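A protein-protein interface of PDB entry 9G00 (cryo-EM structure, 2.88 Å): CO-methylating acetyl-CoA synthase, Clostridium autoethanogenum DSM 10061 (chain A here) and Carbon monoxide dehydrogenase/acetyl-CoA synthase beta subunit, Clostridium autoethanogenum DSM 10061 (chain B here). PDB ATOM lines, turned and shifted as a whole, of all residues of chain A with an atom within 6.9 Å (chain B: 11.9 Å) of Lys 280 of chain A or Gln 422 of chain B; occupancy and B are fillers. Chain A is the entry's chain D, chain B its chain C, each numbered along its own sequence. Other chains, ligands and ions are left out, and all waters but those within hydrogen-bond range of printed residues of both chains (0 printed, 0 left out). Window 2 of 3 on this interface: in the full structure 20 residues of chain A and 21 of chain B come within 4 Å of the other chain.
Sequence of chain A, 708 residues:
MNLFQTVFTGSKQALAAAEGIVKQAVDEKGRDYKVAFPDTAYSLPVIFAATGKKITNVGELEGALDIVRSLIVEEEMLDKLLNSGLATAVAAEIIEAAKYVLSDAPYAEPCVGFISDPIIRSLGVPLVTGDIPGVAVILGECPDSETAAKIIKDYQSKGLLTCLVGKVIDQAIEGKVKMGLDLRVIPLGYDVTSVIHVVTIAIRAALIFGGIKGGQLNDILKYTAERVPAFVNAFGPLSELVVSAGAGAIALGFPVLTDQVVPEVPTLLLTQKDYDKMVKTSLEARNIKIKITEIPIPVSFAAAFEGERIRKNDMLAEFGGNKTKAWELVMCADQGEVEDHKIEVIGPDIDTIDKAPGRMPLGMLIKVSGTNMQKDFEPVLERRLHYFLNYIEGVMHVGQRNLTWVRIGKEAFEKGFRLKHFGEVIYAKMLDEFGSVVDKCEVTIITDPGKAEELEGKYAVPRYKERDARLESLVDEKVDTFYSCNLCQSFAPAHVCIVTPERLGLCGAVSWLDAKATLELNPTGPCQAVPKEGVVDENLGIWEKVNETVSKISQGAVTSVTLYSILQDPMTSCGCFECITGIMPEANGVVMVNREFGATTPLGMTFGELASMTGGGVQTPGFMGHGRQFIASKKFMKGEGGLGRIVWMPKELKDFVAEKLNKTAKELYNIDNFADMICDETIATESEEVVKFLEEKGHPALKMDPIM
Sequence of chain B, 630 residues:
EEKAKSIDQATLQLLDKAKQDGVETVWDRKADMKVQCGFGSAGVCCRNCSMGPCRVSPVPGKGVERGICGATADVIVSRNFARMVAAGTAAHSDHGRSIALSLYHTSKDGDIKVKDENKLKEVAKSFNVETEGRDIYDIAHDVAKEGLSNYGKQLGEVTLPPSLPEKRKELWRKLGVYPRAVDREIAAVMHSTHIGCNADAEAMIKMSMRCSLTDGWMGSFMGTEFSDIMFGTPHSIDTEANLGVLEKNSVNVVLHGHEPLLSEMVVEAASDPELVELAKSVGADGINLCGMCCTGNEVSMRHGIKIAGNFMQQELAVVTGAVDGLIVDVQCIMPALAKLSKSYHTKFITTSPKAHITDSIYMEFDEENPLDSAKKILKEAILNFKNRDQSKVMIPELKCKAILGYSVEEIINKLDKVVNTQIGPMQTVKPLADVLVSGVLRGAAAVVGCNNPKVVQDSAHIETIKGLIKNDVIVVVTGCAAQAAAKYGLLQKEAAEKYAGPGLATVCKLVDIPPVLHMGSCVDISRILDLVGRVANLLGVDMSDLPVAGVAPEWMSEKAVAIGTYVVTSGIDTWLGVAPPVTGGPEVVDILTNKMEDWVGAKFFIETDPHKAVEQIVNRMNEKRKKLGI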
ATOM      1  N   LYS A 150      -9.572  28.525  -9.887  1.00  0.00           N
ATOM      2  CA  LYS A 150      -8.382  27.802 -10.322  1.00  0.00           C
ATOM      3  C   LYS A 150      -7.586  27.304  -9.124  1.00  0.00           C
ATOM      4  O   LYS A 150      -7.201  26.130  -9.072  1.00  0.00           O
ATOM      5  CB  LYS A 150      -7.529  28.705 -11.217  1.00  0.00           C
ATOM      6  CG  LYS A 150      -6.241  28.043 -11.737  1.00  0.00           C
ATOM      7  CD  LYS A 150      -5.042  28.297 -10.797  1.00  0.00           C
ATOM      8  CE  LYS A 150      -3.947  27.238 -10.999  1.00  0.00           C
ATOM      9  NZ  LYS A 150      -2.935  27.248  -9.886  1.00  0.00           N
ATOM     10  N   ASP A 154      -7.318  23.461  -7.994  1.00  0.00           N
ATOM     11  CA  ASP A 154      -5.977  22.884  -7.959  1.00  0.00           C
ATOM     12  C   ASP A 154      -5.728  22.125  -6.651  1.00  0.00           C
ATOM     13  O   ASP A 154      -5.284  20.957  -6.658  1.00  0.00           O
ATOM     14  CB  ASP A 154      -4.965  24.017  -8.157  1.00  0.00           C
ATOM     15  CG  ASP A 154      -3.555  23.517  -8.382  1.00  0.00           C
ATOM     16  OD1 ASP A 154      -3.372  22.286  -8.387  1.00  0.00           O
ATOM     17  OD2 ASP A 154      -2.640  24.342  -8.559  1.00  0.00           O
ATOM     18  N   TYR A 155      -6.121  22.721  -5.519  1.00  0.00           N
ATOM     19  CA  TYR A 155      -6.019  22.002  -4.242  1.00  0.00           C
ATOM     20  C   TYR A 155      -6.916  20.760  -4.214  1.00  0.00           C
ATOM     21  O   TYR A 155      -6.509  19.661  -3.759  1.00  0.00           O
ATOM     22  CB  TYR A 155      -6.401  22.943  -3.087  1.00  0.00           C
ATOM     23  CG  TYR A 155      -5.348  23.960  -2.729  1.00  0.00           C
ATOM     24  CD1 TYR A 155      -4.026  23.572  -2.494  1.00  0.00           C
ATOM     25  CD2 TYR A 155      -5.668  25.314  -2.614  1.00  0.00           C
ATOM     26  CE1 TYR A 155      -3.052  24.502  -2.163  1.00  0.00           C
ATOM     27  CE2 TYR A 155      -4.705  26.253  -2.284  1.00  0.00           C
ATOM     28  CZ  TYR A 155      -3.404  25.826  -2.060  1.00  0.00           C
ATOM     29  OH  TYR A 155      -2.460  26.751  -1.742  1.00  0.00           O
ATOM     30  N   LYS A 158      -5.596  17.843  -6.063  1.00  0.00           N
ATOM     31  CA  LYS A 158      -4.464  17.226  -5.382  1.00  0.00           C
ATOM     32  C   LYS A 158      -4.876  16.460  -4.134  1.00  0.00           C
ATOM     33  O   LYS A 158      -4.008  15.928  -3.429  1.00  0.00           O
ATOM     34  CB  LYS A 158      -3.426  18.280  -5.010  1.00  0.00           C
ATOM     35  CG  LYS A 158      -2.752  18.888  -6.224  1.00  0.00           C
ATOM     36  CD  LYS A 158      -1.579  19.764  -5.795  1.00  0.00           C
ATOM     37  CE  LYS A 158      -1.022  20.565  -6.973  1.00  0.00           C
ATOM     38  NZ  LYS A 158      -0.637  19.682  -8.121  1.00  0.00           N
ATOM     39  N   GLN A 272       3.218  35.878  -1.628  1.00  0.00           N
ATOM     40  CA  GLN A 272       3.325  35.293  -2.961  1.00  0.00           C
ATOM     41  C   GLN A 272       2.249  35.973  -3.803  1.00  0.00           C
ATOM     42  O   GLN A 272       1.062  35.664  -3.668  1.00  0.00           O
ATOM     43  CB  GLN A 272       3.142  33.774  -2.924  1.00  0.00           C
ATOM     44  CG  GLN A 272       3.131  33.115  -4.313  1.00  0.00           C
ATOM     45  CD  GLN A 272       4.424  33.390  -5.080  1.00  0.00           C
ATOM     46  OE1 GLN A 272       4.491  34.321  -5.870  1.00  0.00           O
ATOM     47  NE2 GLN A 272       5.461  32.586  -4.830  1.00  0.00           N
ATOM     48  N   ASP A 274       2.173  35.896  -7.197  1.00  0.00           N
ATOM     49  CA  ASP A 274       1.902  35.069  -8.372  1.00  0.00           C
ATOM     50  C   ASP A 274       0.880  34.001  -8.015  1.00  0.00           C
ATOM     51  O   ASP A 274       1.195  33.011  -7.348  1.00  0.00           O
ATOM     52  CB  ASP A 274       3.203  34.463  -8.883  1.00  0.00           C
ATOM     53  CG  ASP A 274       3.062  33.812 -10.257  1.00  0.00           C
ATOM     54  OD1 ASP A 274       1.940  33.794 -10.798  1.00  0.00           O
ATOM     55  OD2 ASP A 274       4.072  33.324 -10.796  1.00  0.00           O
ATOM     56  N   TYR A 275      -0.364  34.191  -8.468  1.00  0.00           N
ATOM     57  CA  TYR A 275      -1.423  33.226  -8.184  1.00  0.00           C
ATOM     58  C   TYR A 275      -1.191  31.896  -8.877  1.00  0.00           C
ATOM     59  O   TYR A 275      -1.748  30.881  -8.449  1.00  0.00           O
ATOM     60  CB  TYR A 275      -2.788  33.796  -8.605  1.00  0.00           C
ATOM     61  CG  TYR A 275      -3.147  35.050  -7.861  1.00  0.00           C
ATOM     62  CD1 TYR A 275      -3.791  34.992  -6.624  1.00  0.00           C
ATOM     63  CD2 TYR A 275      -2.822  36.306  -8.375  1.00  0.00           C
ATOM     64  CE1 TYR A 275      -4.111  36.153  -5.920  1.00  0.00           C
ATOM     65  CE2 TYR A 275      -3.135  37.476  -7.685  1.00  0.00           C
ATOM     66  CZ  TYR A 275      -3.775  37.387  -6.463  1.00  0.00           C
ATOM     67  OH  TYR A 275      -4.076  38.558  -5.796  1.00  0.00           O
ATOM     68  N   ASP A 276      -0.384  31.875  -9.934  1.00  0.00           N
ATOM     69  CA  ASP A 276      -0.055  30.630 -10.613  1.00  0.00           C
ATOM     70  C   ASP A 276       0.915  29.766  -9.831  1.00  0.00           C
ATOM     71  O   ASP A 276       1.066  28.586 -10.153  1.00  0.00           O
ATOM     72  CB  ASP A 276       0.524  30.920 -11.998  1.00  0.00           C
ATOM     73  CG  ASP A 276      -0.519  31.418 -12.975  1.00  0.00           C
ATOM     74  OD1 ASP A 276      -1.696  31.035 -12.810  1.00  0.00           O
ATOM     75  OD2 ASP A 276      -0.176  32.187 -13.892  1.00  0.00           O
ATOM     76  N   LYS A 277       1.545  30.311  -8.797  1.00  0.00           N
ATOM     77  CA  LYS A 277       2.486  29.564  -7.977  1.00  0.00           C
ATOM     78  C   LYS A 277       2.078  29.476  -6.514  1.00  0.00           C
ATOM     79  O   LYS A 277       2.840  28.939  -5.714  1.00  0.00           O
ATOM     80  CB  LYS A 277       3.885  30.185  -8.073  1.00  0.00           C
ATOM     81  CG  LYS A 277       4.498  30.109  -9.472  1.00  0.00           C
ATOM     82  CD  LYS A 277       6.003  30.428  -9.430  1.00  0.00           C
ATOM     83  CE  LYS A 277       6.260  31.792  -8.772  1.00  0.00           C
ATOM     84  NZ  LYS A 277       7.722  32.115  -8.713  1.00  0.00           N
ATOM     85  N   MET A 278       0.896  29.980  -6.151  1.00  0.00           N
ATOM     86  CA  MET A 278       0.483  29.982  -4.749  1.00  0.00           C
ATOM     87  C   MET A 278       0.309  28.567  -4.207  1.00  0.00           C
ATOM     88  O   MET A 278       0.711  28.280  -3.076  1.00  0.00           O
ATOM     89  CB  MET A 278      -0.810  30.790  -4.583  1.00  0.00           C
ATOM     90  CG  MET A 278      -1.386  30.761  -3.152  1.00  0.00           C
ATOM     91  SD  MET A 278      -0.219  31.340  -1.898  1.00  0.00           S
ATOM     92  CE  MET A 278      -0.357  33.119  -2.036  1.00  0.00           C
ATOM     93  N   VAL A 279      -0.279  27.667  -4.998  1.00  0.00           N
ATOM     94  CA  VAL A 279      -0.447  26.282  -4.557  1.00  0.00           C
ATOM     95  C   VAL A 279       0.909  25.624  -4.312  1.00  0.00           C
ATOM     96  O   VAL A 279       1.142  25.013  -3.260  1.00  0.00           O
ATOM     97  CB  VAL A 279      -1.285  25.502  -5.586  1.00  0.00           C
ATOM     98  CG1 VAL A 279      -1.256  23.995  -5.314  1.00  0.00           C
ATOM     99  CG2 VAL A 279      -2.736  26.010  -5.603  1.00  0.00           C
ATOM    100  N   LYS A 280       1.847  25.786  -5.247  1.00  0.00           N
ATOM    101  CA  LYS A 280       3.170  25.179  -5.065  1.00  0.00           C
ATOM    102  C   LYS A 280       3.925  25.824  -3.906  1.00  0.00           C
ATOM    103  O   LYS A 280       4.615  25.130  -3.140  1.00  0.00           O
ATOM    104  CB  LYS A 280       3.994  25.291  -6.353  1.00  0.00           C
ATOM    105  CG  LYS A 280       3.625  24.265  -7.439  1.00  0.00           C
ATOM    106  CD  LYS A 280       2.175  24.440  -7.942  1.00  0.00           C
ATOM    107  CE  LYS A 280       1.972  25.817  -8.604  1.00  0.00           C
ATOM    108  NZ  LYS A 280       0.537  26.074  -8.923  1.00  0.00           N
ATOM    109  N   THR A 281       3.759  27.135  -3.719  1.00  0.00           N
ATOM    110  CA  THR A 281       4.392  27.798  -2.589  1.00  0.00           C
ATOM    111  C   THR A 281       3.853  27.250  -1.279  1.00  0.00           C
ATOM    112  O   THR A 281       4.614  27.027  -0.332  1.00  0.00           O
ATOM    113  CB  THR A 281       4.139  29.308  -2.675  1.00  0.00           C
ATOM    114  OG1 THR A 281       4.431  29.778  -3.998  1.00  0.00           O
ATOM    115  CG2 THR A 281       4.974  30.081  -1.648  1.00  0.00           C
ATOM    116  N   SER A 282       2.539  27.022  -1.205  1.00  0.00           N
ATOM    117  CA  SER A 282       1.954  26.546   0.045  1.00  0.00           C
ATOM    118  C   SER A 282       2.387  25.118   0.344  1.00  0.00           C
ATOM    119  O   SER A 282       2.683  24.778   1.491  1.00  0.00           O
ATOM    120  CB  SER A 282       0.425  26.634  -0.008  1.00  0.00           C
ATOM    121  OG  SER A 282      -0.015  27.965  -0.253  1.00  0.00           O
ATOM    122  N   LEU A 283       2.433  24.267  -0.684  1.00  0.00           N
ATOM    123  CA  LEU A 283       2.837  22.881  -0.462  1.00  0.00           C
ATOM    124  C   LEU A 283       4.270  22.815   0.039  1.00  0.00           C
ATOM    125  O   LEU A 283       4.589  22.028   0.936  1.00  0.00           O
ATOM    126  CB  LEU A 283       2.669  22.057  -1.740  1.00  0.00           C
ATOM    127  CG  LEU A 283       1.241  22.030  -2.313  1.00  0.00           C
ATOM    128  CD1 LEU A 283       1.208  21.191  -3.582  1.00  0.00           C
ATOM    129  CD2 LEU A 283       0.206  21.524  -1.301  1.00  0.00           C
ATOM    130  N   GLU A 284       5.152  23.638  -0.535  1.00  0.00           N
ATOM    131  CA  GLU A 284       6.518  23.696  -0.024  1.00  0.00           C
ATOM    132  C   GLU A 284       6.569  24.258   1.392  1.00  0.00           C
ATOM    133  O   GLU A 284       7.307  23.746   2.239  1.00  0.00           O
ATOM    134  CB  GLU A 284       7.409  24.523  -0.948  1.00  0.00           C
ATOM    135  CG  GLU A 284       8.833  24.651  -0.404  1.00  0.00           C
ATOM    136  CD  GLU A 284       9.720  25.514  -1.276  1.00  0.00           C
ATOM    137  OE1 GLU A 284       9.322  25.800  -2.418  1.00  0.00           O
ATOM    138  OE2 GLU A 284      10.809  25.911  -0.815  1.00  0.00           O
ATOM    139  N   ALA A 285       5.777  25.293   1.675  1.00  0.00           N
ATOM    140  CA  ALA A 285       5.809  25.926   2.989  1.00  0.00           C
ATOM    141  C   ALA A 285       5.285  25.001   4.076  1.00  0.00           C
ATOM    142  O   ALA A 285       5.741  25.071   5.217  1.00  0.00           O
ATOM    143  CB  ALA A 285       5.016  27.240   2.976  1.00  0.00           C
ATOM    144  N   LYS A 440      13.170  16.836  -5.242  1.00  0.00           N
ATOM    145  CA  LYS A 440      12.961  17.104  -6.656  1.00  0.00           C
ATOM    146  C   LYS A 440      13.919  16.256  -7.473  1.00  0.00           C
ATOM    147  O   LYS A 440      15.063  16.031  -7.071  1.00  0.00           O
ATOM    148  CB  LYS A 440      13.182  18.583  -6.969  1.00  0.00           C
ATOM    149  CG  LYS A 440      12.319  19.528  -6.140  1.00  0.00           C
ATOM    150  CD  LYS A 440      12.545  20.985  -6.526  1.00  0.00           C
ATOM    151  CE  LYS A 440      13.969  21.434  -6.232  1.00  0.00           C
ATOM    152  NZ  LYS A 440      14.220  22.833  -6.665  1.00  0.00           N
ATOM    153  N   ASP B 416      19.726  30.549   3.317  1.00  0.00           N
ATOM    154  CA  ASP B 416      19.033  29.967   2.173  1.00  0.00           C
ATOM    155  C   ASP B 416      18.075  28.846   2.565  1.00  0.00           C
ATOM    156  O   ASP B 416      17.136  28.566   1.817  1.00  0.00           O
ATOM    157  CB  ASP B 416      20.040  29.429   1.152  1.00  0.00           C
ATOM    158  CG  ASP B 416      20.604  30.511   0.250  1.00  0.00           C
ATOM    159  OD1 ASP B 416      20.280  31.697   0.470  1.00  0.00           O
ATOM    160  OD2 ASP B 416      21.368  30.183  -0.675  1.00  0.00           O
ATOM    161  N   LYS B 417      18.262  28.225   3.729  1.00  0.00           N
ATOM    162  CA  LYS B 417      17.379  27.130   4.118  1.00  0.00           C
ATOM    163  C   LYS B 417      15.955  27.613   4.360  1.00  0.00           C
ATOM    164  O   LYS B 417      14.999  26.895   4.056  1.00  0.00           O
ATOM    165  CB  LYS B 417      17.925  26.419   5.359  1.00  0.00           C
ATOM    166  CG  LYS B 417      16.915  25.443   5.960  1.00  0.00           C
ATOM    167  CD  LYS B 417      17.569  24.487   6.950  1.00  0.00           C
ATOM    168  CE  LYS B 417      18.084  25.248   8.163  1.00  0.00           C
ATOM    169  NZ  LYS B 417      17.968  24.393   9.378  1.00  0.00           N
ATOM    170  N   VAL B 418      15.783  28.811   4.922  1.00  0.00           N
ATOM    171  CA  VAL B 418      14.458  29.298   5.300  1.00  0.00           C
ATOM    172  C   VAL B 418      13.839  30.108   4.156  1.00  0.00           C
ATOM    173  O   VAL B 418      12.861  30.832   4.359  1.00  0.00           O
ATOM    174  CB  VAL B 418      14.500  30.127   6.601  1.00  0.00           C
ATOM    175  CG1 VAL B 418      14.957  29.260   7.788  1.00  0.00           C
ATOM    176  CG2 VAL B 418      15.389  31.371   6.451  1.00  0.00           C
ATOM    177  N   VAL B 419      14.383  29.979   2.945  1.00  0.00           N
ATOM    178  CA  VAL B 419      13.851  30.657   1.765  1.00  0.00           C
ATOM    179  C   VAL B 419      12.917  29.695   1.036  1.00  0.00           C
ATOM    180  O   VAL B 419      13.335  28.604   0.626  1.00  0.00           O
ATOM    181  CB  VAL B 419      14.976  31.141   0.832  1.00  0.00           C
ATOM    182  CG1 VAL B 419      14.387  31.734  -0.455  1.00  0.00           C
ATOM    183  CG2 VAL B 419      15.870  32.175   1.529  1.00  0.00           C
ATOM    184  N   ASN B 420      11.667  30.107   0.838  1.00  0.00           N
ATOM    185  CA  ASN B 420      10.750  29.321   0.022  1.00  0.00           C
ATOM    186  C   ASN B 420      11.233  29.346  -1.424  1.00  0.00           C
ATOM    187  O   ASN B 420      11.441  30.416  -2.001  1.00  0.00           O
ATOM    188  CB  ASN B 420       9.321  29.859   0.134  1.00  0.00           C
ATOM    189  CG  ASN B 420       8.278  28.898  -0.455  1.00  0.00           C
ATOM    190  OD1 ASN B 420       8.172  28.768  -1.667  1.00  0.00           O
ATOM    191  ND2 ASN B 420       7.508  28.224   0.407  1.00  0.00           N
ATOM    192  N   THR B 421      11.385  28.158  -2.020  1.00  0.00           N
ATOM    193  CA  THR B 421      11.937  28.061  -3.370  1.00  0.00           C
ATOM    194  C   THR B 421      11.041  28.763  -4.377  1.00  0.00           C
ATOM    195  O   THR B 421      11.531  29.388  -5.320  1.00  0.00           O
ATOM    196  CB  THR B 421      12.133  26.594  -3.766  1.00  0.00           C
ATOM    197  OG1 THR B 421      13.077  25.960  -2.892  1.00  0.00           O
ATOM    198  CG2 THR B 421      12.652  26.484  -5.187  1.00  0.00           C
ATOM    199  N   GLN B 422       9.725  28.656  -4.207  1.00  0.00           N
ATOM    200  CA  GLN B 422       8.786  29.278  -5.133  1.00  0.00           C
ATOM    201  C   GLN B 422       8.758  30.800  -5.021  1.00  0.00           C
ATOM    202  O   GLN B 422       8.155  31.452  -5.881  1.00  0.00           O
ATOM    203  CB  GLN B 422       7.371  28.725  -4.906  1.00  0.00           C
ATOM    204  CG  GLN B 422       7.273  27.191  -4.987  1.00  0.00           C
ATOM    205  CD  GLN B 422       7.717  26.650  -6.343  1.00  0.00           C
ATOM    206  OE1 GLN B 422       7.259  27.112  -7.379  1.00  0.00           O
ATOM    207  NE2 GLN B 422       8.626  25.673  -6.336  1.00  0.00           N
ATOM    208  N   ILE B 423       9.361  31.382  -3.986  1.00  0.00           N
ATOM    209  CA  ILE B 423       9.389  32.832  -3.797  1.00  0.00           C
ATOM    210  C   ILE B 423      10.773  33.399  -4.100  1.00  0.00           C
ATOM    211  O   ILE B 423      10.933  34.224  -5.000  1.00  0.00           O
ATOM    212  CB  ILE B 423       8.921  33.219  -2.374  1.00  0.00           C
ATOM    213  CG1 ILE B 423       7.497  32.701  -2.116  1.00  0.00           C
ATOM    214  CG2 ILE B 423       8.998  34.743  -2.189  1.00  0.00           C
ATOM    215  CD1 ILE B 423       7.052  32.851  -0.665  1.00  0.00           C
ATOM    216  N   GLY B 424      11.786  32.973  -3.351  1.00  0.00           N
ATOM    217  CA  GLY B 424      13.123  33.489  -3.488  1.00  0.00           C
ATOM    218  C   GLY B 424      13.222  34.929  -3.021  1.00  0.00           C
ATOM    219  O   GLY B 424      12.333  35.437  -2.337  1.00  0.00           O
ATOM    220  N   PRO B 425      14.318  35.612  -3.374  1.00  0.00           N
ATOM    221  CA  PRO B 425      15.487  35.116  -4.123  1.00  0.00           C
ATOM    222  C   PRO B 425      16.426  34.329  -3.221  1.00  0.00           C
ATOM    223  O   PRO B 425      16.267  34.323  -2.004  1.00  0.00           O
ATOM    224  CB  PRO B 425      16.124  36.414  -4.654  1.00  0.00           C
ATOM    225  CG  PRO B 425      15.844  37.417  -3.544  1.00  0.00           C
ATOM    226  CD  PRO B 425      14.460  37.041  -3.024  1.00  0.00           C
ATOM    227  N   MET B 426      17.387  33.625  -3.807  1.00  0.00           N
ATOM    228  CA  MET B 426      18.388  32.893  -3.053  1.00  0.00           C
ATOM    229  C   MET B 426      19.663  33.722  -2.949  1.00  0.00           C
ATOM    230  O   MET B 426      19.864  34.699  -3.677  1.00  0.00           O
ATOM    231  CB  MET B 426      18.688  31.541  -3.723  1.00  0.00           C
ATOM    232  CG  MET B 426      17.500  30.548  -3.709  1.00  0.00           C
ATOM    233  SD  MET B 426      17.091  29.988  -2.045  1.00  0.00           S
ATOM    234  CE  MET B 426      15.722  28.881  -2.348  1.00  0.00           C
ATOM    235  N   LYS B 430      18.229  38.562   2.634  1.00  0.00           N
ATOM    236  CA  LYS B 430      16.816  38.886   2.782  1.00  0.00           C
ATOM    237  C   LYS B 430      16.136  38.182   3.950  1.00  0.00           C
ATOM    238  O   LYS B 430      15.324  38.835   4.625  1.00  0.00           O
ATOM    239  CB  LYS B 430      16.069  38.591   1.482  1.00  0.00           C
ATOM    240  CG  LYS B 430      14.624  39.075   1.512  1.00  0.00           C
ATOM    241  CD  LYS B 430      13.963  38.879   0.155  1.00  0.00           C
ATOM    242  CE  LYS B 430      12.591  39.553   0.110  1.00  0.00           C
ATOM    243  NZ  LYS B 430      11.670  38.985   1.155  1.00  0.00           N
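The backbone carbonyl oxygen (O) of Gln 422 of chain B lies within hydrogen-bond range of the side-chain amide nitrogen (NE2) of Gln 272 of chain A (3.1 Å).
The side-chain carboxylate of Glu 284 of chain A sits at hydrogen-bond distance from the backbone NH of Gln 422 of chain B, at 3.4 Å.
The side-chain amide oxygen (OD1) of Asn 420 of chain B sits close to the side-chain carboxylate (OE1) of Glu 284 of chain A (3.3 Å).
O of Thr 281 of chain A lies within hydrogen-bond range of ND2 of Asn 420 of chain B, 3.2 Å away.
The side-chain carboxylate (OE2) of Glu 284 of chain A is in hydrogen-bond range of the backbone NH (N) of Thr 421 of chain B, 2.6 Å away.
The side-chain amino group of Lys 277 of chain A sits at hydrogen-bond distance from the backbone carbonyl oxygen of Gln 422 of chain B, at 2.9 Å.
The backbone carbonyl oxygen (O) of Lys 277 of chain A sits at hydrogen-bond distance from the side-chain hydroxyl (OG1) of Thr 281 of chain A, at 2.5 Å.
The backbone NH of Asp 274 of chain A is in hydrogen-bond range of the side-chain amide oxygen of Gln 272 of chain A (3.1 Å).
The side-chain hydroxyl of Thr 281 of chain A lies within hydrogen-bond range of the side-chain amide nitrogen of Gln 272 of chain A (3.1 Å).
O of Asp 276 of chain A sits at hydrogen-bond distance from NZ of Lys 280 of chain A, 2.8 Å away.
The side-chain amino group (NZ) of Lys 280 of chain A is in salt-bridge range of the side-chain carboxylate (OD2) of Asp 154 of chain A (3.6 Å).
The backbone NH (N) of Gln 422 of chain B sits at hydrogen-bond distance from the side-chain amide oxygen (OD1) of Asn 420 of chain B, 3.0 Å away.
Among the printed residues, merely in contact across the chains: Thr 281 of chain A with Gln 422 of chain B, Gln 272 of chain A with Ile 423 of chain B, Thr 281 of chain A with Ile 423 of chain B, Ala 285 of chain A with Asn 420 of chain B, Lys 280 of chain A with Gln 422 of chain B and Glu 284 of chain A with Val 419 of chain B.
Lys 150 of chain A touches none of the printed residues of chain B.
Tyr 275 of chain A touches none of the printed residues of chain B.
Lys 277 of chain A touches just one residue of chain B: Gln 422.
Val 279 of chain A touches none of the printed residues of chain B.
No residue of chain B comes within 4 Å of Ser 282 of chain A.
Leu 283 of chain A touches none of the printed residues of chain B.
Glu 284 of chain A touches four residues of chain B.
Printed residues of chain A within 4 Å of Val 419 of chain B: Glu 284.
Printed residues of chain A within 4 Å of Thr 421 of chain B: Glu 284 (2.6 Å).
Gln 422 of chain B touches just these residues of chain A: Gln 272, Lys 277, Lys 280, Thr 281 and Glu 284.
The nearest residue of chain B that does not touch Lys 280 of chain A is Asn 420 of chain B (5.3 Å).
The nearest residue of chain A that does not touch Gln 422 of chain B is Ser 282 of chain A (6.1 Å).
Hydrophobic or aromatic side chains of chain A that line the printed part of chain B: Ala 285.
Among the printed residues, 12 pairs touch across the chains.
Among the printed residues, no Asp or Glu carboxylate lies within 4 Å of a Lys or Arg side-chain nitrogen of the other chain.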
